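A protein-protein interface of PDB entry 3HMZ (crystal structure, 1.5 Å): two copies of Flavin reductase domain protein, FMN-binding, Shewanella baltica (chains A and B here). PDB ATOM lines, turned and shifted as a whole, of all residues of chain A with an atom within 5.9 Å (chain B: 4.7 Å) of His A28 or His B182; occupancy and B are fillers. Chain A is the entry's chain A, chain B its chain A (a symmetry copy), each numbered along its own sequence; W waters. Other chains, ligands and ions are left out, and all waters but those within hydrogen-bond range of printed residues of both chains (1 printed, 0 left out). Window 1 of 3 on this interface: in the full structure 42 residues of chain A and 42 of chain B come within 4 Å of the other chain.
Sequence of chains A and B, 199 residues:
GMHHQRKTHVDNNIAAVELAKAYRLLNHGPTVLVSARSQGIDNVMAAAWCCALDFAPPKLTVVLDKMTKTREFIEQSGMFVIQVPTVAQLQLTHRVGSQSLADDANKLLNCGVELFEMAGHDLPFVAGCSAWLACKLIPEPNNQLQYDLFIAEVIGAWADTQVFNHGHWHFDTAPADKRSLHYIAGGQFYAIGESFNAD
ND2 of Asn A27 lies within hydrogen-bond range of O of Ile B184 (2.8 Å). A ring nitrogen (ND1) of His B182 is in hydrogen-bond range of the backbone carbonyl oxygen (O) of His A28 (3.0 Å). The backbone NH (N) of His A28 sits at hydrogen-bond distance from the backbone carbonyl oxygen (O) of Tyr B183. The side-chain hydroxyl (OH) of Tyr B190 is in hydrogen-bond range of the backbone carbonyl oxygen (O) of Trp A169 (3.0 Å). N of Phe A171 sits at hydrogen-bond distance from OH of Tyr B190. ND1 of His A182 sits at hydrogen-bond distance from O of His B28, at 3.0 Å. The backbone carbonyl oxygen (O) of Asn A27 sits close to the backbone carbonyl oxygen (O) of Tyr B183. The backbone carbonyl oxygen (O) of His A28 sits close to the backbone carbonyl oxygen (O) of Gly B29 (3.3 Å). O of His B28 sits close to O of Gly A29 (3.3 Å).
OG of Ser A180 is in hydrogen-bond range of NE2 of His A28. The side-chain hydroxyl of Ser A180 is in hydrogen-bond range of a ring nitrogen (NE2) of His A182 (2.8 Å). The backbone carbonyl oxygen of Ser A180 lies within hydrogen-bond range of the backbone NH of Ile A192, 3.0 Å away. OG of Ser B180 lies within hydrogen-bond range of NE2 of His B28, at 3.0 Å. The side-chain hydroxyl of Thr B31 is in hydrogen-bond range of the backbone NH of Tyr B183 (3.0 Å). The side-chain hydroxyl of Ser B180 lies within hydrogen-bond range of a ring nitrogen (NE2) of His B182 (2.8 Å).
Among the printed residues, pairs that only touch across the chains: Arg A24 with Ile B184, His A28 with Ile B184, Gly A29 with Gly B29, Trp A169 with Ile B184, His A182 with Ile B192, Ile A192 with His B182, Ile A192 with Tyr B190 and Ile A192 with Ala B191.
Of the printed residues of chain A, His B28 touches Gly A29 (3.3 Å) and His A182 (3.0 Å). Printed residues of chain A within 4 Å of His B182: His A28 (3.0 Å) and Ile A192 (3.9 Å). Of the printed residues of chain A, Tyr B190 touches Trp A169 (3.0 Å), Phe A171 (3.5 Å) and Ile A192 (3.6 Å). Printed residues of chain A within 4 Å of Ile B192: His A182. The nearest residue of chain A that does not touch His B182 is His A182 (4.3 Å). The nearest printed residue of chain A that does not touch Tyr B190 is His A28 (4.9 Å).
Of the 13 printed residues of chain A, 8 touch a printed residue of chain B. Printed residues of chain B that touch a printed residue of chain A: His B28, Gly B29, His B182, Tyr B183, Ile B184, Tyr B190, Ala B191 and Ile B192. Along chain B the printed residues that touch a printed residue of chain A span positions 28 to 192. Among the printed residues, 17 pairs touch across the chains. Among the printed residues, no Asp or Glu carboxylate lies within 4 Å of a Lys or Arg side-chain nitrogen of the other chain.
His A28 touches Gly B29, and with the chains exchanged Gly A29 touches His B28. His A28 touches His B182, and with the chains exchanged His A182 touches His B28. Gly A29 touches its own counterpart, Gly B29. His A182 touches Ile B192, and with the chains exchanged Ile A192 touches His B182. Positions printed for both chains: 28, 29, 30, 180, 182 and 192. Of the 17 pairs that touch across the chains among the printed residues, 7 have their exchanged pair printed and touching as well.
Water W1 lies within hydrogen-bond range of OG1 of Thr B31 (2.8 Å), O of Asn A27 (2.8 Å) and O of Gly B29 (2.9 Å).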
ATOM      1  N   ARG A  24      31.527  -2.256 -33.143  1.00  0.00           N
ATOM      2  CA  ARG A  24      30.501  -2.695 -32.182  1.00  0.00           C
ATOM      3  C   ARG A  24      29.222  -3.206 -32.855  1.00  0.00           C
ATOM      4  O   ARG A  24      28.475  -3.983 -32.281  1.00  0.00           O
ATOM      5  CB  ARG A  24      30.160  -1.592 -31.211  1.00  0.00           C
ATOM      6  CG  ARG A  24      31.340  -1.242 -30.326  1.00  0.00           C
ATOM      7  CD  ARG A  24      30.952  -0.250 -29.333  1.00  0.00           C
ATOM      8  NE  ARG A  24      32.085   0.184 -28.517  1.00  0.00           N
ATOM      9  CZ  ARG A  24      31.983   1.103 -27.571  1.00  0.00           C
ATOM     10  NH1 ARG A  24      30.838   1.729 -27.357  1.00  0.00           N
ATOM     11  NH2 ARG A  24      33.062   1.439 -26.873  1.00  0.00           N
ATOM     12  N   LEU A  25      29.005  -2.779 -34.102  1.00  0.00           N
ATOM     13  CA  LEU A  25      27.851  -3.208 -34.861  1.00  0.00           C
ATOM     14  C   LEU A  25      27.894  -4.728 -35.126  1.00  0.00           C
ATOM     15  O   LEU A  25      26.857  -5.336 -35.407  1.00  0.00           O
ATOM     16  CB  LEU A  25      27.757  -2.435 -36.189  1.00  0.00           C
ATOM     17  CG  LEU A  25      27.565  -0.921 -36.011  1.00  0.00           C
ATOM     18  CD1 LEU A  25      27.714  -0.166 -37.353  1.00  0.00           C
ATOM     19  CD2 LEU A  25      26.224  -0.573 -35.335  1.00  0.00           C
ATOM     20  N   LEU A  26      29.097  -5.322 -35.127  1.00  0.00           N
ATOM     21  CA  LEU A  26      29.267  -6.732 -35.418  1.00  0.00           C
ATOM     22  C   LEU A  26      29.795  -7.541 -34.241  1.00  0.00           C
ATOM     23  O   LEU A  26      30.031  -8.731 -34.389  1.00  0.00           O
ATOM     24  CB  LEU A  26      30.227  -6.912 -36.598  1.00  0.00           C
ATOM     25  CG  LEU A  26      29.825  -6.241 -37.899  1.00  0.00           C
ATOM     26  CD1 LEU A  26      30.869  -6.468 -38.974  1.00  0.00           C
ATOM     27  CD2 LEU A  26      28.427  -6.699 -38.373  1.00  0.00           C
ATOM     28  N   ASN A  27      30.052  -6.891 -33.101  1.00  0.00           N
ATOM     29  CA  ASN A  27      30.798  -7.545 -32.018  1.00  0.00           C
ATOM     30  C   ASN A  27      30.108  -8.761 -31.412  1.00  0.00           C
ATOM     31  O   ASN A  27      30.780  -9.720 -31.025  1.00  0.00           O
ATOM     32  CB  ASN A  27      31.192  -6.530 -30.953  1.00  0.00           C
ATOM     33  CG  ASN A  27      32.655  -6.568 -30.613  1.00  0.00           C
ATOM     34  OD1 ASN A  27      33.477  -6.905 -31.440  1.00  0.00           O
ATOM     35  ND2 ASN A  27      32.985  -6.138 -29.413  1.00  0.00           N
ATOM     36  N   HIS A  28      28.774  -8.716 -31.404  1.00  0.00           N
ATOM     37  CA  HIS A  28      27.953  -9.795 -30.900  1.00  0.00           C
ATOM     38  C   HIS A  28      27.773 -10.963 -31.904  1.00  0.00           C
ATOM     39  O   HIS A  28      27.052 -11.919 -31.623  1.00  0.00           O
ATOM     40  CB  HIS A  28      26.615  -9.271 -30.409  1.00  0.00           C
ATOM     41  CG  HIS A  28      25.785  -8.640 -31.468  1.00  0.00           C
ATOM     42  ND1 HIS A  28      26.217  -7.564 -32.222  1.00  0.00           N
ATOM     43  CD2 HIS A  28      24.511  -8.879 -31.836  1.00  0.00           C
ATOM     44  CE1 HIS A  28      25.253  -7.214 -33.057  1.00  0.00           C
ATOM     45  NE2 HIS A  28      24.207  -8.004 -32.850  1.00  0.00           N
ATOM     46  N   GLY A  29      28.448 -10.879 -33.064  1.00  0.00           N
ATOM     47  CA  GLY A  29      28.482 -11.931 -34.050  1.00  0.00           C
ATOM     48  C   GLY A  29      27.188 -12.224 -34.818  1.00  0.00           C
ATOM     49  O   GLY A  29      26.886 -13.384 -35.108  1.00  0.00           O
ATOM     50  N   PRO A  30      26.467 -11.180 -35.237  1.00  0.00           N
ATOM     51  CA  PRO A  30      25.257 -11.455 -36.001  1.00  0.00           C
ATOM     52  C   PRO A  30      25.556 -12.022 -37.394  1.00  0.00           C
ATOM     53  O   PRO A  30      26.602 -11.749 -37.974  1.00  0.00           O
ATOM     54  CB  PRO A  30      24.646 -10.055 -36.180  1.00  0.00           C
ATOM     55  CG  PRO A  30      25.857  -9.121 -36.222  1.00  0.00           C
ATOM     56  CD  PRO A  30      26.765  -9.736 -35.195  1.00  0.00           C
ATOM     57  N   VAL A  84      23.229  -5.554 -40.938  1.00  0.00           N
ATOM     58  CA  VAL A  84      22.703  -6.416 -39.892  1.00  0.00           C
ATOM     59  C   VAL A  84      21.198  -6.538 -40.027  1.00  0.00           C
ATOM     60  O   VAL A  84      20.480  -5.574 -39.731  1.00  0.00           O
ATOM     61  CB  VAL A  84      23.095  -5.859 -38.497  1.00  0.00           C
ATOM     62  CG1 VAL A  84      22.601  -6.782 -37.412  1.00  0.00           C
ATOM     63  CG2 VAL A  84      24.649  -5.693 -38.360  1.00  0.00           C
ATOM     64  N   TRP A 169      24.306  -0.933 -28.575  1.00  0.00           N
ATOM     65  CA  TRP A 169      23.069  -1.575 -28.921  1.00  0.00           C
ATOM     66  C   TRP A 169      22.093  -1.385 -27.779  1.00  0.00           C
ATOM     67  O   TRP A 169      22.508  -1.287 -26.604  1.00  0.00           O
ATOM     68  CB  TRP A 169      23.258  -3.077 -29.177  1.00  0.00           C
ATOM     69  CG  TRP A 169      23.957  -3.382 -30.447  1.00  0.00           C
ATOM     70  CD1 TRP A 169      25.248  -3.694 -30.597  1.00  0.00           C
ATOM     71  CD2 TRP A 169      23.381  -3.381 -31.765  1.00  0.00           C
ATOM     72  NE1 TRP A 169      25.540  -3.955 -31.920  1.00  0.00           N
ATOM     73  CE2 TRP A 169      24.412  -3.729 -32.669  1.00  0.00           C
ATOM     74  CE3 TRP A 169      22.112  -3.101 -32.265  1.00  0.00           C
ATOM     75  CZ2 TRP A 169      24.199  -3.856 -34.032  1.00  0.00           C
ATOM     76  CZ3 TRP A 169      21.904  -3.207 -33.644  1.00  0.00           C
ATOM     77  CH2 TRP A 169      22.943  -3.603 -34.498  1.00  0.00           C
ATOM     78  N   PHE A 171      19.000  -3.461 -27.678  1.00  0.00           N
ATOM     79  CA  PHE A 171      17.984  -4.488 -28.017  1.00  0.00           C
ATOM     80  C   PHE A 171      16.893  -4.637 -26.945  1.00  0.00           C
ATOM     81  O   PHE A 171      15.715  -4.920 -27.275  1.00  0.00           O
ATOM     82  CB  PHE A 171      18.648  -5.844 -28.264  1.00  0.00           C
ATOM     83  CG  PHE A 171      19.523  -5.878 -29.444  1.00  0.00           C
ATOM     84  CD1 PHE A 171      18.988  -5.742 -30.730  1.00  0.00           C
ATOM     85  CD2 PHE A 171      20.890  -6.142 -29.324  1.00  0.00           C
ATOM     86  CE1 PHE A 171      19.825  -5.832 -31.837  1.00  0.00           C
ATOM     87  CE2 PHE A 171      21.687  -6.230 -30.423  1.00  0.00           C
ATOM     88  CZ  PHE A 171      21.163  -6.082 -31.680  1.00  0.00           C
ATOM     89  N   SER A 180      18.886  -8.833 -33.717  1.00  0.00           N
ATOM     90  CA  SER A 180      19.698  -9.465 -34.740  1.00  0.00           C
ATOM     91  C   SER A 180      19.477 -10.979 -34.755  1.00  0.00           C
ATOM     92  O   SER A 180      18.982 -11.563 -33.783  1.00  0.00           O
ATOM     93  CB  SER A 180      21.177  -9.126 -34.545  1.00  0.00           C
ATOM     94  OG  SER A 180      21.628  -9.411 -33.213  1.00  0.00           O
ATOM     95  N   HIS A 182      21.142 -14.829 -35.632  1.00  0.00           N
ATOM     96  CA  HIS A 182      22.384 -15.591 -35.430  1.00  0.00           C
ATOM     97  C   HIS A 182      22.127 -17.003 -35.918  1.00  0.00           C
ATOM     98  O   HIS A 182      21.457 -17.782 -35.269  1.00  0.00           O
ATOM     99  CB  HIS A 182      22.800 -15.505 -33.955  1.00  0.00           C
ATOM    100  CG  HIS A 182      22.990 -14.098 -33.467  1.00  0.00           C
ATOM    101  ND1 HIS A 182      24.236 -13.557 -33.234  1.00  0.00           N
ATOM    102  CD2 HIS A 182      22.105 -13.089 -33.273  1.00  0.00           C
ATOM    103  CE1 HIS A 182      24.096 -12.288 -32.876  1.00  0.00           C
ATOM    104  NE2 HIS A 182      22.814 -11.973 -32.930  1.00  0.00           N
ATOM    105  N   ILE A 192      19.228 -12.420 -30.885  1.00  0.00           N
ATOM    106  CA  ILE A 192      20.014 -12.001 -29.748  1.00  0.00           C
ATOM    107  C   ILE A 192      19.043 -11.862 -28.549  1.00  0.00           C
ATOM    108  O   ILE A 192      17.857 -11.538 -28.717  1.00  0.00           O
ATOM    109  CB  ILE A 192      20.755 -10.676 -30.073  1.00  0.00           C
ATOM    110  CG1 ILE A 192      21.944 -10.434 -29.134  1.00  0.00           C
ATOM    111  CG2 ILE A 192      19.803  -9.464 -30.135  1.00  0.00           C
ATOM    112  CD1 ILE A 192      22.998 -11.596 -29.122  1.00  0.00           C
ATOM    113  N   HIS B  28      26.498 -19.042 -34.616  1.00  0.00           N
ATOM    114  CA  HIS B  28      25.742 -17.951 -34.042  1.00  0.00           C
ATOM    115  C   HIS B  28      26.624 -16.789 -33.518  1.00  0.00           C
ATOM    116  O   HIS B  28      26.111 -15.823 -32.955  1.00  0.00           O
ATOM    117  CB  HIS B  28      24.794 -18.458 -32.969  1.00  0.00           C
ATOM    118  CG  HIS B  28      25.474 -19.087 -31.807  1.00  0.00           C
ATOM    119  ND1 HIS B  28      26.323 -20.173 -31.929  1.00  0.00           N
ATOM    120  CD2 HIS B  28      25.358 -18.839 -30.488  1.00  0.00           C
ATOM    121  CE1 HIS B  28      26.748 -20.519 -30.725  1.00  0.00           C
ATOM    122  NE2 HIS B  28      26.184 -19.717 -29.831  1.00  0.00           N
ATOM    123  N   GLY B  29      27.950 -16.888 -33.726  1.00  0.00           N
ATOM    124  CA  GLY B  29      28.892 -15.843 -33.409  1.00  0.00           C
ATOM    125  C   GLY B  29      29.142 -15.542 -31.927  1.00  0.00           C
ATOM    126  O   GLY B  29      29.314 -14.381 -31.548  1.00  0.00           O
ATOM    127  N   PRO B  30      29.260 -16.582 -31.095  1.00  0.00           N
ATOM    128  CA  PRO B  30      29.537 -16.300 -29.693  1.00  0.00           C
ATOM    129  C   PRO B  30      30.949 -15.746 -29.471  1.00  0.00           C
ATOM    130  O   PRO B  30      31.866 -16.033 -30.233  1.00  0.00           O
ATOM    131  CB  PRO B  30      29.468 -17.694 -29.049  1.00  0.00           C
ATOM    132  CG  PRO B  30      29.937 -18.641 -30.156  1.00  0.00           C
ATOM    133  CD  PRO B  30      29.314 -18.028 -31.378  1.00  0.00           C
ATOM    134  N   THR B  31      31.097 -15.020 -28.380  1.00  0.00           N
ATOM    135  CA  THR B  31      32.397 -14.667 -27.849  1.00  0.00           C
ATOM    136  C   THR B  31      32.939 -15.971 -27.244  1.00  0.00           C
ATOM    137  O   THR B  31      32.190 -16.750 -26.656  1.00  0.00           O
ATOM    138  CB  THR B  31      32.259 -13.544 -26.834  1.00  0.00           C
ATOM    139  OG1 THR B  31      31.850 -12.371 -27.553  1.00  0.00           O
ATOM    140  CG2 THR B  31      33.536 -13.298 -26.117  1.00  0.00           C
ATOM    141  N   SER B 180      25.074 -18.839 -24.563  1.00  0.00           N
ATOM    142  CA  SER B 180      26.328 -18.223 -24.954  1.00  0.00           C
ATOM    143  C   SER B 180      26.277 -16.707 -24.753  1.00  0.00           C
ATOM    144  O   SER B 180      25.198 -16.112 -24.649  1.00  0.00           O
ATOM    145  CB  SER B 180      26.678 -18.576 -26.401  1.00  0.00           C
ATOM    146  OG  SER B 180      25.603 -18.287 -27.305  1.00  0.00           O
ATOM    147  N   LEU B 181      27.468 -16.129 -24.661  1.00  0.00           N
ATOM    148  CA  LEU B 181      27.693 -14.726 -24.479  1.00  0.00           C
ATOM    149  C   LEU B 181      28.227 -14.102 -25.750  1.00  0.00           C
ATOM    150  O   LEU B 181      29.057 -14.678 -26.427  1.00  0.00           O
ATOM    151  CB  LEU B 181      28.708 -14.495 -23.370  1.00  0.00           C
ATOM    152  CG  LEU B 181      28.278 -14.800 -21.939  1.00  0.00           C
ATOM    153  CD1 LEU B 181      29.525 -14.819 -20.986  1.00  0.00           C
ATOM    154  CD2 LEU B 181      27.239 -13.775 -21.470  1.00  0.00           C
ATOM    155  N   HIS B 182      27.737 -12.881 -26.014  1.00  0.00           N
ATOM    156  CA  HIS B 182      28.006 -12.131 -27.251  1.00  0.00           C
ATOM    157  C   HIS B 182      28.383 -10.719 -26.844  1.00  0.00           C
ATOM    158  O   HIS B 182      27.543  -9.929 -26.460  1.00  0.00           O
ATOM    159  CB  HIS B 182      26.782 -12.210 -28.172  1.00  0.00           C
ATOM    160  CG  HIS B 182      26.381 -13.615 -28.516  1.00  0.00           C
ATOM    161  ND1 HIS B 182      26.609 -14.167 -29.758  1.00  0.00           N
ATOM    162  CD2 HIS B 182      25.869 -14.614 -27.754  1.00  0.00           C
ATOM    163  CE1 HIS B 182      26.212 -15.432 -29.748  1.00  0.00           C
ATOM    164  NE2 HIS B 182      25.795 -15.735 -28.531  1.00  0.00           N
ATOM    165  N   TYR B 183      29.676 -10.453 -26.838  1.00  0.00           N
ATOM    166  CA  TYR B 183      30.196  -9.195 -26.301  1.00  0.00           C
ATOM    167  C   TYR B 183      29.926  -7.987 -27.141  1.00  0.00           C
ATOM    168  O   TYR B 183      29.959  -8.072 -28.357  1.00  0.00           O
ATOM    169  CB  TYR B 183      31.705  -9.320 -26.165  1.00  0.00           C
ATOM    170  CG  TYR B 183      32.414  -8.198 -25.474  1.00  0.00           C
ATOM    171  CD1 TYR B 183      32.053  -7.833 -24.199  1.00  0.00           C
ATOM    172  CD2 TYR B 183      33.558  -7.615 -26.038  1.00  0.00           C
ATOM    173  CE1 TYR B 183      32.748  -6.833 -23.504  1.00  0.00           C
ATOM    174  CE2 TYR B 183      34.270  -6.625 -25.338  1.00  0.00           C
ATOM    175  CZ  TYR B 183      33.868  -6.262 -24.073  1.00  0.00           C
ATOM    176  OH  TYR B 183      34.609  -5.308 -23.388  1.00  0.00           O
ATOM    177  N   ILE B 184      29.684  -6.852 -26.484  1.00  0.00           N
ATOM    178  CA  ILE B 184      29.687  -5.557 -27.198  1.00  0.00           C
ATOM    179  C   ILE B 184      30.872  -4.705 -26.759  1.00  0.00           C
ATOM    180  O   ILE B 184      31.804  -4.461 -27.562  1.00  0.00           O
ATOM    181  CB  ILE B 184      28.367  -4.784 -27.058  1.00  0.00           C
ATOM    182  CG1 ILE B 184      27.214  -5.600 -27.636  1.00  0.00           C
ATOM    183  CG2 ILE B 184      28.496  -3.433 -27.757  1.00  0.00           C
ATOM    184  CD1 ILE B 184      27.388  -5.983 -29.134  1.00  0.00           C
ATOM    185  N   PHE B 189      27.535  -7.607 -22.381  1.00  0.00           N
ATOM    186  CA  PHE B 189      27.302  -8.716 -23.283  1.00  0.00           C
ATOM    187  C   PHE B 189      25.808  -8.935 -23.441  1.00  0.00           C
ATOM    188  O   PHE B 189      25.004  -8.516 -22.617  1.00  0.00           O
ATOM    189  CB  PHE B 189      27.822 -10.031 -22.678  1.00  0.00           C
ATOM    190  CG  PHE B 189      29.310 -10.079 -22.368  1.00  0.00           C
ATOM    191  CD1 PHE B 189      29.835  -9.433 -21.235  1.00  0.00           C
ATOM    192  CD2 PHE B 189      30.169 -10.871 -23.124  1.00  0.00           C
ATOM    193  CE1 PHE B 189      31.186  -9.490 -20.930  1.00  0.00           C
ATOM    194  CE2 PHE B 189      31.549 -10.962 -22.799  1.00  0.00           C
ATOM    195  CZ  PHE B 189      32.038 -10.290 -21.695  1.00  0.00           C
ATOM    196  N   TYR B 190      25.449  -9.579 -24.529  1.00  0.00           N
ATOM    197  CA  TYR B 190      24.115 -10.139 -24.693  1.00  0.00           C
ATOM    198  C   TYR B 190      24.231 -11.654 -24.679  1.00  0.00           C
ATOM    199  O   TYR B 190      25.154 -12.232 -25.258  1.00  0.00           O
ATOM    200  CB  TYR B 190      23.457  -9.728 -25.994  1.00  0.00           C
ATOM    201  CG  TYR B 190      23.100  -8.306 -26.056  1.00  0.00           C
ATOM    202  CD1 TYR B 190      21.970  -7.838 -25.436  1.00  0.00           C
ATOM    203  CD2 TYR B 190      23.885  -7.412 -26.763  1.00  0.00           C
ATOM    204  CE1 TYR B 190      21.636  -6.461 -25.471  1.00  0.00           C
ATOM    205  CE2 TYR B 190      23.565  -6.071 -26.840  1.00  0.00           C
ATOM    206  CZ  TYR B 190      22.438  -5.596 -26.192  1.00  0.00           C
ATOM    207  OH  TYR B 190      22.101  -4.255 -26.270  1.00  0.00           O
ATOM    208  N   ALA B 191      23.294 -12.295 -23.996  1.00  0.00           N
ATOM    209  CA  ALA B 191      23.129 -13.738 -24.090  1.00  0.00           C
ATOM    210  C   ALA B 191      22.384 -14.045 -25.378  1.00  0.00           C
ATOM    211  O   ALA B 191      21.595 -13.226 -25.870  1.00  0.00           O
ATOM    212  CB  ALA B 191      22.339 -14.279 -22.882  1.00  0.00           C
ATOM    213  N   ILE B 192      22.594 -15.237 -25.933  1.00  0.00           N
ATOM    214  CA  ILE B 192      21.815 -15.656 -27.075  1.00  0.00           C
ATOM    215  C   ILE B 192      20.345 -15.777 -26.604  1.00  0.00           C
ATOM    216  O   ILE B 192      20.068 -16.090 -25.435  1.00  0.00           O
ATOM    217  CB  ILE B 192      22.373 -16.991 -27.638  1.00  0.00           C
ATOM    218  CG1 ILE B 192      21.926 -17.238 -29.086  1.00  0.00           C
ATOM    219  CG2 ILE B 192      22.074 -18.193 -26.720  1.00  0.00           C
ATOM    220  CD1 ILE B 192      22.309 -16.088 -30.080  1.00  0.00           C
HETATM  221  O   HOH W   1      30.245 -12.262 -29.862  1.00  0.00           O
